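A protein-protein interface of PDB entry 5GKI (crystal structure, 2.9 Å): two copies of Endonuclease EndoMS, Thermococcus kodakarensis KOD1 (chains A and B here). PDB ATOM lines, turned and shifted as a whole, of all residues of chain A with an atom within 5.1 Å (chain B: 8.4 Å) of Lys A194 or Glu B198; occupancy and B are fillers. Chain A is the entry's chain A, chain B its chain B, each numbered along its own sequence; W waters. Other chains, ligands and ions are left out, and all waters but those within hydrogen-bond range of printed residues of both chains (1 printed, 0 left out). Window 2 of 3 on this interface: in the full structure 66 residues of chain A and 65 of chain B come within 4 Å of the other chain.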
ATOM      1  N   VAL A 190      -9.576  13.733  11.385  1.00  0.00           N
ATOM      2  CA  VAL A 190      -8.886  13.730  10.105  1.00  0.00           C
ATOM      3  C   VAL A 190      -9.915  13.444   9.013  1.00  0.00           C
ATOM      4  O   VAL A 190      -9.808  13.956   7.907  1.00  0.00           O
ATOM      5  CB  VAL A 190      -7.711  12.727  10.085  1.00  0.00           C
ATOM      6  CG1 VAL A 190      -7.082  12.685   8.724  1.00  0.00           C
ATOM      7  CG2 VAL A 190      -6.649  13.140  11.105  1.00  0.00           C
ATOM      8  N   ARG A 191     -10.948  12.681   9.352  1.00  0.00           N
ATOM      9  CA  ARG A 191     -12.037  12.424   8.417  1.00  0.00           C
ATOM     10  C   ARG A 191     -12.809  13.697   8.120  1.00  0.00           C
ATOM     11  O   ARG A 191     -13.183  13.948   6.978  1.00  0.00           O
ATOM     12  CB  ARG A 191     -12.983  11.353   8.961  1.00  0.00           C
ATOM     13  CG  ARG A 191     -12.371   9.961   9.056  1.00  0.00           C
ATOM     14  CD  ARG A 191     -13.457   8.918   9.169  1.00  0.00           C
ATOM     15  NE  ARG A 191     -12.972   7.724   9.842  1.00  0.00           N
ATOM     16  CZ  ARG A 191     -13.098   7.533  11.146  1.00  0.00           C
ATOM     17  NH1 ARG A 191     -13.707   8.452  11.879  1.00  0.00           N
ATOM     18  NH2 ARG A 191     -12.628   6.437  11.712  1.00  0.00           N
ATOM     19  N   GLN A 192     -13.051  14.486   9.159  1.00  0.00           N
ATOM     20  CA  GLN A 192     -13.664  15.801   9.016  1.00  0.00           C
ATOM     21  C   GLN A 192     -12.839  16.662   8.054  1.00  0.00           C
ATOM     22  O   GLN A 192     -13.343  17.159   7.048  1.00  0.00           O
ATOM     23  CB  GLN A 192     -13.769  16.489  10.382  1.00  0.00           C
ATOM     24  CG  GLN A 192     -15.131  16.449  11.074  1.00  0.00           C
ATOM     25  CD  GLN A 192     -15.124  17.220  12.405  1.00  0.00           C
ATOM     26  OE1 GLN A 192     -14.948  16.614  13.459  1.00  0.00           O
ATOM     27  NE2 GLN A 192     -15.305  18.562  12.353  1.00  0.00           N
ATOM     28  N   LEU A 193     -11.563  16.827   8.376  1.00  0.00           N
ATOM     29  CA  LEU A 193     -10.664  17.620   7.558  1.00  0.00           C
ATOM     30  C   LEU A 193     -10.711  17.154   6.100  1.00  0.00           C
ATOM     31  O   LEU A 193     -11.126  17.902   5.231  1.00  0.00           O
ATOM     32  CB  LEU A 193      -9.249  17.542   8.112  1.00  0.00           C
ATOM     33  CG  LEU A 193      -8.220  18.406   7.396  1.00  0.00           C
ATOM     34  CD1 LEU A 193      -8.736  19.846   7.295  1.00  0.00           C
ATOM     35  CD2 LEU A 193      -6.839  18.325   8.082  1.00  0.00           C
ATOM     36  N   LYS A 194     -10.310  15.912   5.844  1.00  0.00           N
ATOM     37  CA  LYS A 194     -10.310  15.342   4.498  1.00  0.00           C
ATOM     38  C   LYS A 194     -11.646  15.545   3.764  1.00  0.00           C
ATOM     39  O   LYS A 194     -11.658  16.013   2.634  1.00  0.00           O
ATOM     40  CB  LYS A 194      -9.952  13.857   4.572  1.00  0.00           C
ATOM     41  CG  LYS A 194     -10.057  13.073   3.271  1.00  0.00           C
ATOM     42  CD  LYS A 194      -9.705  11.601   3.506  1.00  0.00           C
ATOM     43  CE  LYS A 194      -9.955  10.741   2.279  1.00  0.00           C
ATOM     44  NZ  LYS A 194     -11.349  10.877   1.792  1.00  0.00           N
ATOM     45  N   SER A 195     -12.758  15.220   4.410  1.00  0.00           N
ATOM     46  CA  SER A 195     -14.081  15.520   3.864  1.00  0.00           C
ATOM     47  C   SER A 195     -14.204  16.990   3.387  1.00  0.00           C
ATOM     48  O   SER A 195     -14.605  17.262   2.249  1.00  0.00           O
ATOM     49  CB  SER A 195     -15.156  15.190   4.919  1.00  0.00           C
ATOM     50  OG  SER A 195     -16.459  15.650   4.582  1.00  0.00           O
ATOM     51  N   TYR A 196     -13.840  17.940   4.238  1.00  0.00           N
ATOM     52  CA  TYR A 196     -13.971  19.344   3.855  1.00  0.00           C
ATOM     53  C   TYR A 196     -13.079  19.674   2.660  1.00  0.00           C
ATOM     54  O   TYR A 196     -13.506  20.342   1.725  1.00  0.00           O
ATOM     55  CB  TYR A 196     -13.639  20.264   5.035  1.00  0.00           C
ATOM     56  CG  TYR A 196     -14.478  19.988   6.261  1.00  0.00           C
ATOM     57  CD1 TYR A 196     -15.789  19.530   6.149  1.00  0.00           C
ATOM     58  CD2 TYR A 196     -13.955  20.164   7.530  1.00  0.00           C
ATOM     59  CE1 TYR A 196     -16.558  19.269   7.281  1.00  0.00           C
ATOM     60  CE2 TYR A 196     -14.711  19.905   8.669  1.00  0.00           C
ATOM     61  CZ  TYR A 196     -16.007  19.461   8.540  1.00  0.00           C
ATOM     62  OH  TYR A 196     -16.737  19.221   9.681  1.00  0.00           O
ATOM     63  N   VAL A 197     -11.846  19.184   2.696  1.00  0.00           N
ATOM     64  CA  VAL A 197     -10.870  19.474   1.656  1.00  0.00           C
ATOM     65  C   VAL A 197     -11.376  18.976   0.312  1.00  0.00           C
ATOM     66  O   VAL A 197     -11.221  19.645  -0.708  1.00  0.00           O
ATOM     67  CB  VAL A 197      -9.493  18.833   1.951  1.00  0.00           C
ATOM     68  CG1 VAL A 197      -8.535  19.109   0.817  1.00  0.00           C
ATOM     69  CG2 VAL A 197      -8.915  19.361   3.243  1.00  0.00           C
ATOM     70  N   GLU A 198     -11.995  17.803   0.319  1.00  0.00           N
ATOM     71  CA  GLU A 198     -12.510  17.217  -0.911  1.00  0.00           C
ATOM     72  C   GLU A 198     -13.530  18.159  -1.517  1.00  0.00           C
ATOM     73  O   GLU A 198     -13.449  18.512  -2.693  1.00  0.00           O
ATOM     74  CB  GLU A 198     -13.127  15.831  -0.654  1.00  0.00           C
ATOM     75  CG  GLU A 198     -12.238  14.682  -1.109  1.00  0.00           C
ATOM     76  CD  GLU A 198     -12.396  13.422  -0.269  1.00  0.00           C
ATOM     77  OE1 GLU A 198     -13.514  13.177   0.240  1.00  0.00           O
ATOM     78  OE2 GLU A 198     -11.392  12.685  -0.114  1.00  0.00           O
ATOM     79  N   ILE A 199     -14.474  18.586  -0.691  1.00  0.00           N
ATOM     80  CA  ILE A 199     -15.579  19.403  -1.155  1.00  0.00           C
ATOM     81  C   ILE A 199     -15.116  20.732  -1.731  1.00  0.00           C
ATOM     82  O   ILE A 199     -15.633  21.187  -2.747  1.00  0.00           O
ATOM     83  CB  ILE A 199     -16.546  19.642  -0.023  1.00  0.00           C
ATOM     84  CG1 ILE A 199     -17.027  18.289   0.497  1.00  0.00           C
ATOM     85  CG2 ILE A 199     -17.678  20.554  -0.469  1.00  0.00           C
ATOM     86  CD1 ILE A 199     -18.215  18.369   1.384  1.00  0.00           C
ATOM     87  N   GLU A 228      -3.268  10.739   3.214  1.00  0.00           N
ATOM     88  CA  GLU A 228      -4.093  11.549   2.326  1.00  0.00           C
ATOM     89  C   GLU A 228      -3.456  12.923   2.054  1.00  0.00           C
ATOM     90  O   GLU A 228      -4.087  13.815   1.488  1.00  0.00           O
ATOM     91  CB  GLU A 228      -5.507  11.688   2.888  1.00  0.00           C
ATOM     92  CG  GLU A 228      -6.535  10.888   2.078  1.00  0.00           C
ATOM     93  CD  GLU A 228      -6.777  11.453   0.662  1.00  0.00           C
ATOM     94  OE1 GLU A 228      -7.001  12.683   0.532  1.00  0.00           O
ATOM     95  OE2 GLU A 228      -6.751  10.665  -0.321  1.00  0.00           O
ATOM     96  N   LEU A 230      -2.288  15.468   4.038  1.00  0.00           N
ATOM     97  CA  LEU A 230      -2.707  16.651   4.757  1.00  0.00           C
ATOM     98  C   LEU A 230      -1.616  17.072   5.750  1.00  0.00           C
ATOM     99  O   LEU A 230      -0.623  16.359   5.911  1.00  0.00           O
ATOM    100  CB  LEU A 230      -4.036  16.383   5.449  1.00  0.00           C
ATOM    101  CG  LEU A 230      -5.247  16.294   4.517  1.00  0.00           C
ATOM    102  CD1 LEU A 230      -6.340  15.396   5.088  1.00  0.00           C
ATOM    103  CD2 LEU A 230      -5.813  17.674   4.300  1.00  0.00           C
ATOM    104  N   ILE B 159      -9.968  -2.892   9.893  1.00  0.00           N
ATOM    105  CA  ILE B 159      -9.247  -2.785   8.644  1.00  0.00           C
ATOM    106  C   ILE B 159      -7.986  -1.990   8.966  1.00  0.00           C
ATOM    107  O   ILE B 159      -7.629  -1.842  10.129  1.00  0.00           O
ATOM    108  CB  ILE B 159     -10.090  -2.131   7.559  1.00  0.00           C
ATOM    109  CG1 ILE B 159     -10.540  -0.748   7.997  1.00  0.00           C
ATOM    110  CG2 ILE B 159     -11.332  -2.964   7.309  1.00  0.00           C
ATOM    111  CD1 ILE B 159     -11.487  -0.130   7.018  1.00  0.00           C
ATOM    112  N   VAL B 177     -19.325  -3.342   3.387  1.00  0.00           N
ATOM    113  CA  VAL B 177     -19.208  -2.635   4.662  1.00  0.00           C
ATOM    114  C   VAL B 177     -20.548  -2.090   5.128  1.00  0.00           C
ATOM    115  O   VAL B 177     -21.258  -1.451   4.358  1.00  0.00           O
ATOM    116  CB  VAL B 177     -18.248  -1.448   4.566  1.00  0.00           C
ATOM    117  CG1 VAL B 177     -18.094  -0.784   5.913  1.00  0.00           C
ATOM    118  CG2 VAL B 177     -16.917  -1.897   4.053  1.00  0.00           C
ATOM    119  N   ARG B 191     -19.259   9.916   6.684  1.00  0.00           N
ATOM    120  CA  ARG B 191     -17.801  10.028   6.645  1.00  0.00           C
ATOM    121  C   ARG B 191     -17.132   8.757   7.165  1.00  0.00           C
ATOM    122  O   ARG B 191     -16.113   8.344   6.635  1.00  0.00           O
ATOM    123  CB  ARG B 191     -17.311  11.228   7.444  1.00  0.00           C
ATOM    124  CG  ARG B 191     -17.842  12.557   6.963  1.00  0.00           C
ATOM    125  CD  ARG B 191     -17.067  13.724   7.566  1.00  0.00           C
ATOM    126  NE  ARG B 191     -17.767  14.979   7.322  1.00  0.00           N
ATOM    127  CZ  ARG B 191     -18.503  15.615   8.225  1.00  0.00           C
ATOM    128  NH1 ARG B 191     -18.609  15.143   9.452  1.00  0.00           N
ATOM    129  NH2 ARG B 191     -19.108  16.744   7.897  1.00  0.00           N
ATOM    130  N   GLN B 192     -17.715   8.124   8.179  1.00  0.00           N
ATOM    131  CA  GLN B 192     -17.147   6.892   8.709  1.00  0.00           C
ATOM    132  C   GLN B 192     -17.146   5.845   7.608  1.00  0.00           C
ATOM    133  O   GLN B 192     -16.095   5.353   7.201  1.00  0.00           O
ATOM    134  CB  GLN B 192     -17.944   6.382   9.909  1.00  0.00           C
ATOM    135  CG  GLN B 192     -17.482   6.879  11.256  1.00  0.00           C
ATOM    136  CD  GLN B 192     -18.048   6.095  12.433  1.00  0.00           C
ATOM    137  OE1 GLN B 192     -18.170   6.644  13.516  1.00  0.00           O
ATOM    138  NE2 GLN B 192     -18.269   4.796  12.267  1.00  0.00           N
ATOM    139  N   LEU B 193     -18.339   5.539   7.110  1.00  0.00           N
ATOM    140  CA  LEU B 193     -18.517   4.554   6.045  1.00  0.00           C
ATOM    141  C   LEU B 193     -17.620   4.840   4.860  1.00  0.00           C
ATOM    142  O   LEU B 193     -16.849   3.984   4.445  1.00  0.00           O
ATOM    143  CB  LEU B 193     -19.972   4.525   5.588  1.00  0.00           C
ATOM    144  CG  LEU B 193     -20.466   3.514   4.548  1.00  0.00           C
ATOM    145  CD1 LEU B 193     -20.207   2.085   5.009  1.00  0.00           C
ATOM    146  CD2 LEU B 193     -21.965   3.730   4.242  1.00  0.00           C
ATOM    147  N   LYS B 194     -17.716   6.060   4.337  1.00  0.00           N
ATOM    148  CA  LYS B 194     -16.924   6.474   3.188  1.00  0.00           C
ATOM    149  C   LYS B 194     -15.437   6.241   3.444  1.00  0.00           C
ATOM    150  O   LYS B 194     -14.719   5.751   2.587  1.00  0.00           O
ATOM    151  CB  LYS B 194     -17.201   7.947   2.844  1.00  0.00           C
ATOM    152  CG  LYS B 194     -16.140   8.589   1.946  1.00  0.00           C
ATOM    153  CD  LYS B 194     -16.657   9.847   1.247  1.00  0.00           C
ATOM    154  CE  LYS B 194     -15.587  10.504   0.362  1.00  0.00           C
ATOM    155  NZ  LYS B 194     -14.489  11.137   1.156  1.00  0.00           N
ATOM    156  N   SER B 195     -14.988   6.565   4.645  1.00  0.00           N
ATOM    157  CA  SER B 195     -13.607   6.317   5.030  1.00  0.00           C
ATOM    158  C   SER B 195     -13.223   4.843   4.947  1.00  0.00           C
ATOM    159  O   SER B 195     -12.155   4.502   4.458  1.00  0.00           O
ATOM    160  CB  SER B 195     -13.370   6.819   6.448  1.00  0.00           C
ATOM    161  OG  SER B 195     -12.031   6.643   6.846  1.00  0.00           O
ATOM    162  N   TYR B 196     -14.089   3.970   5.444  1.00  0.00           N
ATOM    163  CA  TYR B 196     -13.790   2.545   5.460  1.00  0.00           C
ATOM    164  C   TYR B 196     -13.750   1.980   4.029  1.00  0.00           C
ATOM    165  O   TYR B 196     -12.882   1.177   3.675  1.00  0.00           O
ATOM    166  CB  TYR B 196     -14.825   1.795   6.306  1.00  0.00           C
ATOM    167  CG  TYR B 196     -14.974   2.296   7.733  1.00  0.00           C
ATOM    168  CD1 TYR B 196     -13.926   2.934   8.407  1.00  0.00           C
ATOM    169  CD2 TYR B 196     -16.176   2.122   8.410  1.00  0.00           C
ATOM    170  CE1 TYR B 196     -14.087   3.385   9.727  1.00  0.00           C
ATOM    171  CE2 TYR B 196     -16.346   2.559   9.707  1.00  0.00           C
ATOM    172  CZ  TYR B 196     -15.305   3.192  10.366  1.00  0.00           C
ATOM    173  OH  TYR B 196     -15.519   3.619  11.661  1.00  0.00           O
ATOM    174  N   VAL B 197     -14.693   2.420   3.208  1.00  0.00           N
ATOM    175  CA  VAL B 197     -14.827   1.919   1.852  1.00  0.00           C
ATOM    176  C   VAL B 197     -13.624   2.279   0.984  1.00  0.00           C
ATOM    177  O   VAL B 197     -13.099   1.431   0.272  1.00  0.00           O
ATOM    178  CB  VAL B 197     -16.117   2.452   1.208  1.00  0.00           C
ATOM    179  CG1 VAL B 197     -16.218   2.017  -0.241  1.00  0.00           C
ATOM    180  CG2 VAL B 197     -17.320   1.959   1.990  1.00  0.00           C
ATOM    181  N   GLU B 198     -13.187   3.530   1.057  1.00  0.00           N
ATOM    182  CA  GLU B 198     -11.982   3.971   0.356  1.00  0.00           C
ATOM    183  C   GLU B 198     -10.802   3.046   0.658  1.00  0.00           C
ATOM    184  O   GLU B 198     -10.145   2.515  -0.250  1.00  0.00           O
ATOM    185  CB  GLU B 198     -11.640   5.423   0.741  1.00  0.00           C
ATOM    186  CG  GLU B 198     -12.405   6.448  -0.079  1.00  0.00           C
ATOM    187  CD  GLU B 198     -12.044   7.873   0.256  1.00  0.00           C
ATOM    188  OE1 GLU B 198     -10.957   8.096   0.831  1.00  0.00           O
ATOM    189  OE2 GLU B 198     -12.855   8.771  -0.058  1.00  0.00           O
ATOM    190  N   ILE B 199     -10.566   2.853   1.947  1.00  0.00           N
ATOM    191  CA  ILE B 199      -9.521   1.983   2.440  1.00  0.00           C
ATOM    192  C   ILE B 199      -9.678   0.538   1.955  1.00  0.00           C
ATOM    193  O   ILE B 199      -8.696  -0.139   1.654  1.00  0.00           O
ATOM    194  CB  ILE B 199      -9.505   2.040   3.964  1.00  0.00           C
ATOM    195  CG1 ILE B 199      -8.976   3.409   4.394  1.00  0.00           C
ATOM    196  CG2 ILE B 199      -8.653   0.940   4.548  1.00  0.00           C
ATOM    197  CD1 ILE B 199      -9.077   3.655   5.864  1.00  0.00           C
ATOM    198  N   LEU B 200     -10.911   0.071   1.851  1.00  0.00           N
ATOM    199  CA  LEU B 200     -11.132  -1.278   1.374  1.00  0.00           C
ATOM    200  C   LEU B 200     -10.974  -1.377  -0.130  1.00  0.00           C
ATOM    201  O   LEU B 200     -10.498  -2.396  -0.630  1.00  0.00           O
ATOM    202  CB  LEU B 200     -12.506  -1.768   1.803  1.00  0.00           C
ATOM    203  CG  LEU B 200     -12.411  -2.190   3.264  1.00  0.00           C
ATOM    204  CD1 LEU B 200     -13.659  -2.909   3.703  1.00  0.00           C
ATOM    205  CD2 LEU B 200     -11.174  -3.065   3.475  1.00  0.00           C
ATOM    206  N   ARG B 201     -11.353  -0.317  -0.846  1.00  0.00           N
ATOM    207  CA  ARG B 201     -11.240  -0.290  -2.304  1.00  0.00           C
ATOM    208  C   ARG B 201      -9.798  -0.551  -2.714  1.00  0.00           C
ATOM    209  O   ARG B 201      -9.547  -1.114  -3.777  1.00  0.00           O
ATOM    210  CB  ARG B 201     -11.727   1.049  -2.887  1.00  0.00           C
ATOM    211  CG  ARG B 201     -13.254   1.244  -2.942  1.00  0.00           C
ATOM    212  CD  ARG B 201     -13.656   2.505  -3.766  1.00  0.00           C
ATOM    213  NE  ARG B 201     -15.000   3.062  -3.494  1.00  0.00           N
ATOM    214  CZ  ARG B 201     -16.158   2.401  -3.647  1.00  0.00           C
ATOM    215  NH1 ARG B 201     -16.164   1.128  -4.041  1.00  0.00           N
ATOM    216  NH2 ARG B 201     -17.325   3.001  -3.389  1.00  0.00           N
ATOM    217  N   GLU B 202      -8.854  -0.159  -1.862  1.00  0.00           N
ATOM    218  CA  GLU B 202      -7.437  -0.399  -2.124  1.00  0.00           C
ATOM    219  C   GLU B 202      -7.139  -1.890  -2.283  1.00  0.00           C
ATOM    220  O   GLU B 202      -6.556  -2.309  -3.281  1.00  0.00           O
ATOM    221  CB  GLU B 202      -6.572   0.181  -1.010  1.00  0.00           C
ATOM    222  CG  GLU B 202      -6.685   1.683  -0.832  1.00  0.00           C
ATOM    223  CD  GLU B 202      -6.111   2.143   0.496  1.00  0.00           C
ATOM    224  OE1 GLU B 202      -5.471   1.313   1.186  1.00  0.00           O
ATOM    225  OE2 GLU B 202      -6.303   3.327   0.850  1.00  0.00           O
ATOM    226  N   GLU B 203      -7.546  -2.692  -1.307  1.00  0.00           N
ATOM    227  CA  GLU B 203      -7.284  -4.119  -1.371  1.00  0.00           C
ATOM    228  C   GLU B 203      -8.206  -4.828  -2.365  1.00  0.00           C
ATOM    229  O   GLU B 203      -7.748  -5.609  -3.189  1.00  0.00           O
ATOM    230  CB  GLU B 203      -7.416  -4.750   0.017  1.00  0.00           C
ATOM    231  CG  GLU B 203      -6.541  -5.986   0.202  1.00  0.00           C
ATOM    232  CD  GLU B 203      -6.282  -6.326   1.663  1.00  0.00           C
ATOM    233  OE1 GLU B 203      -7.255  -6.428   2.442  1.00  0.00           O
ATOM    234  OE2 GLU B 203      -5.098  -6.489   2.034  1.00  0.00           O
ATOM    235  N   TYR B 204      -9.504  -4.568  -2.278  1.00  0.00           N
ATOM    236  CA  TYR B 204     -10.478  -5.351  -3.027  1.00  0.00           C
ATOM    237  C   TYR B 204     -11.004  -4.724  -4.327  1.00  0.00           C
ATOM    238  O   TYR B 204     -11.765  -5.360  -5.061  1.00  0.00           O
ATOM    239  CB  TYR B 204     -11.663  -5.675  -2.116  1.00  0.00           C
ATOM    240  CG  TYR B 204     -11.310  -6.525  -0.913  1.00  0.00           C
ATOM    241  CD1 TYR B 204     -10.919  -5.949   0.287  1.00  0.00           C
ATOM    242  CD2 TYR B 204     -11.377  -7.901  -0.976  1.00  0.00           C
ATOM    243  CE1 TYR B 204     -10.601  -6.731   1.385  1.00  0.00           C
ATOM    244  CE2 TYR B 204     -11.066  -8.690   0.116  1.00  0.00           C
ATOM    245  CZ  TYR B 204     -10.676  -8.106   1.291  1.00  0.00           C
ATOM    246  OH  TYR B 204     -10.365  -8.913   2.367  1.00  0.00           O
ATOM    247  N   GLY B 205     -10.610  -3.495  -4.628  1.00  0.00           N
ATOM    248  CA  GLY B 205     -11.102  -2.853  -5.837  1.00  0.00           C
ATOM    249  C   GLY B 205     -12.420  -2.106  -5.699  1.00  0.00           C
ATOM    250  O   GLY B 205     -12.877  -1.839  -4.590  1.00  0.00           O
ATOM    251  N   ASP B 206     -13.039  -1.783  -6.833  1.00  0.00           N
ATOM    252  CA  ASP B 206     -14.286  -1.010  -6.866  1.00  0.00           C
ATOM    253  C   ASP B 206     -15.524  -1.865  -6.611  1.00  0.00           C
ATOM    254  O   ASP B 206     -16.638  -1.359  -6.656  1.00  0.00           O
ATOM    255  CB  ASP B 206     -14.462  -0.305  -8.216  1.00  0.00           C
ATOM    256  CG  ASP B 206     -13.319   0.625  -8.550  1.00  0.00           C
ATOM    257  OD1 ASP B 206     -12.739   1.218  -7.609  1.00  0.00           O
ATOM    258  OD2 ASP B 206     -13.018   0.764  -9.762  1.00  0.00           O
ATOM    259  N   VAL B 208     -16.460  -3.028  -3.899  1.00  0.00           N
ATOM    260  CA  VAL B 208     -16.917  -2.716  -2.543  1.00  0.00           C
ATOM    261  C   VAL B 208     -18.121  -1.773  -2.402  1.00  0.00           C
ATOM    262  O   VAL B 208     -18.149  -0.677  -2.965  1.00  0.00           O
ATOM    263  CB  VAL B 208     -15.764  -2.090  -1.750  1.00  0.00           C
ATOM    264  CG1 VAL B 208     -16.129  -1.984  -0.289  1.00  0.00           C
ATOM    265  CG2 VAL B 208     -14.492  -2.888  -1.943  1.00  0.00           C
ATOM    266  N   GLY B 210     -20.396   0.315   0.406  1.00  0.00           N
ATOM    267  CA  GLY B 210     -20.781   0.721   1.745  1.00  0.00           C
ATOM    268  C   GLY B 210     -22.290   0.832   1.895  1.00  0.00           C
ATOM    269  O   GLY B 210     -22.962   1.430   1.058  1.00  0.00           O
ATOM    270  N   LYS B 227     -23.806  11.284  -3.294  1.00  0.00           N
ATOM    271  CA  LYS B 227     -22.687  11.829  -4.061  1.00  0.00           C
ATOM    272  C   LYS B 227     -21.540  10.815  -4.156  1.00  0.00           C
ATOM    273  O   LYS B 227     -20.805  10.761  -5.148  1.00  0.00           O
ATOM    274  CB  LYS B 227     -22.191  13.144  -3.438  1.00  0.00           C
ATOM    275  CG  LYS B 227     -20.997  13.793  -4.156  1.00  0.00           C
ATOM    276  CD  LYS B 227     -20.548  15.092  -3.476  1.00  0.00           C
ATOM    277  CE  LYS B 227     -19.493  14.850  -2.390  1.00  0.00           C
ATOM    278  NZ  LYS B 227     -18.330  14.043  -2.871  1.00  0.00           N
ATOM    279  N   GLU B 228     -21.385  10.011  -3.116  1.00  0.00           N
ATOM    280  CA  GLU B 228     -20.296   9.047  -3.080  1.00  0.00           C
ATOM    281  C   GLU B 228     -20.728   7.641  -3.531  1.00  0.00           C
ATOM    282  O   GLU B 228     -19.966   6.671  -3.433  1.00  0.00           O
ATOM    283  CB  GLU B 228     -19.676   9.032  -1.686  1.00  0.00           C
ATOM    284  CG  GLU B 228     -18.915  10.329  -1.367  1.00  0.00           C
ATOM    285  CD  GLU B 228     -17.683  10.570  -2.257  1.00  0.00           C
ATOM    286  OE1 GLU B 228     -17.313   9.686  -3.066  1.00  0.00           O
ATOM    287  OE2 GLU B 228     -17.075  11.660  -2.134  1.00  0.00           O
ATOM    288  N   LEU B 230     -23.060   5.483  -2.329  1.00  0.00           N
ATOM    289  CA  LEU B 230     -23.194   4.504  -1.275  1.00  0.00           C
ATOM    290  C   LEU B 230     -24.663   4.258  -1.055  1.00  0.00           C
ATOM    291  O   LEU B 230     -25.500   4.924  -1.655  1.00  0.00           O
ATOM    292  CB  LEU B 230     -22.515   4.986   0.004  1.00  0.00           C
ATOM    293  CG  LEU B 230     -20.999   5.183  -0.059  1.00  0.00           C
ATOM    294  CD1 LEU B 230     -20.502   6.155   0.983  1.00  0.00           C
ATOM    295  CD2 LEU B 230     -20.336   3.846   0.153  1.00  0.00           C
HETATM  296  O   HOH W   1     -13.619  10.980   4.277  1.00  0.00           O
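Printed residues of chain A that touch a printed residue of chain B: Arg A191, Lys A194, Ser A195, Tyr A196 and Glu A198.
Hydrophobic or aromatic side chains of chain A that line the printed part of chain B: Tyr A196.
Of the 23 printed residues of chain B, 5 touch a printed residue of chain A.
Hydrophobic or aromatic side chains of chain B that line the printed part of chain A: Tyr B196.
Among the printed residues, 8 pairs touch across the chains.
Among the printed residues, Asp or Glu carboxylates within 4 Å of a Lys or Arg side-chain nitrogen of the other chain: Lys A194 with Glu B198 and Glu A198 with Lys B194.
The side-chain amino group of Lys A194 sits close to the side-chain amino group of Lys B194 (3.2 Å).
OE1 of Glu A198 is in salt-bridge range of NZ of Lys B194 (2.4 Å).
The side-chain hydroxyl (OG) of Ser A195 lies within hydrogen-bond range of the guanidinium group (NE) of Arg B191, at 3.1 Å.
The side-chain amino group of Lys A194 is in salt-bridge range of the side-chain carboxylate of Glu B198, at 3.0 Å.
The guanidinium group (NE) of Arg A191 lies within hydrogen-bond range of the side-chain hydroxyl (OG) of Ser B195.
Water W1 bridges the side-chain amino group (NZ) of Lys B194 and the side-chain amino group (NZ) of Lys A194.
Of chain B, only Lys B194 (3.2 Å) and Glu B198 (3.0 Å) come within 4 Å of Lys A194.
Of chain A, only Lys A194 (3.0 Å) comes within 4 Å of Glu B198.
Of the printed residues of chain A, Ser B195 touches Arg A191 (3.3 Å).
Of the printed residues of chain B, Ser A195 touches Arg B191.
Of the printed residues of chain B, Tyr A196 touches Arg B191 (3.6 Å).
Of the printed residues of chain A, Lys B194 touches Lys A194 and Glu A198.
Val B208 touches none of the printed residues of chain A.
Tyr B204 touches none of the printed residues of chain A.
The nearest residue of chain B that does not touch Lys A194 is Ser B195 (6.0 Å).
The nearest residue of chain A that does not touch Glu B198 is Glu A198 (4.2 Å).
The nearest printed residue of chain B that does not touch Tyr A196 is Lys B194 (7.5 Å).
Arg A191 touches its own counterpart, Arg B191.
Arg A191 touches Ser B195, and with the chains exchanged Ser A195 touches Arg B191.
Arg A191 touches Tyr B196, and with the chains exchanged Tyr A196 touches Arg B191.
Lys A194 touches Glu B198, and with the chains exchanged Glu A198 touches Lys B194.
Positions printed for both chains: 191, 192, 193, 194, 195, 196, 197, 198, 199, 228 and 230.
The side-chain amide nitrogen of Gln B192 lies within hydrogen-bond range of the side-chain hydroxyl of Tyr B196, 3.1 Å away.
OE2 of Glu B198 lies within salt-bridge range of NZ of Lys B194, at 3.1 Å.
OH of Tyr A196 is in hydrogen-bond range of NE2 of Gln A192 (3.1 Å).
The side-chain carboxylate (OE2) of Glu A198 lies within salt-bridge range of the side-chain amino group (NZ) of Lys A194.
Arg A191 touches Arg B191.
Arg A191 touches Tyr B196 (NH2 to CE1, 3.9 Å).
NH2 of Arg B191 touches CE1 of Tyr A196, at 3.6 Å.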
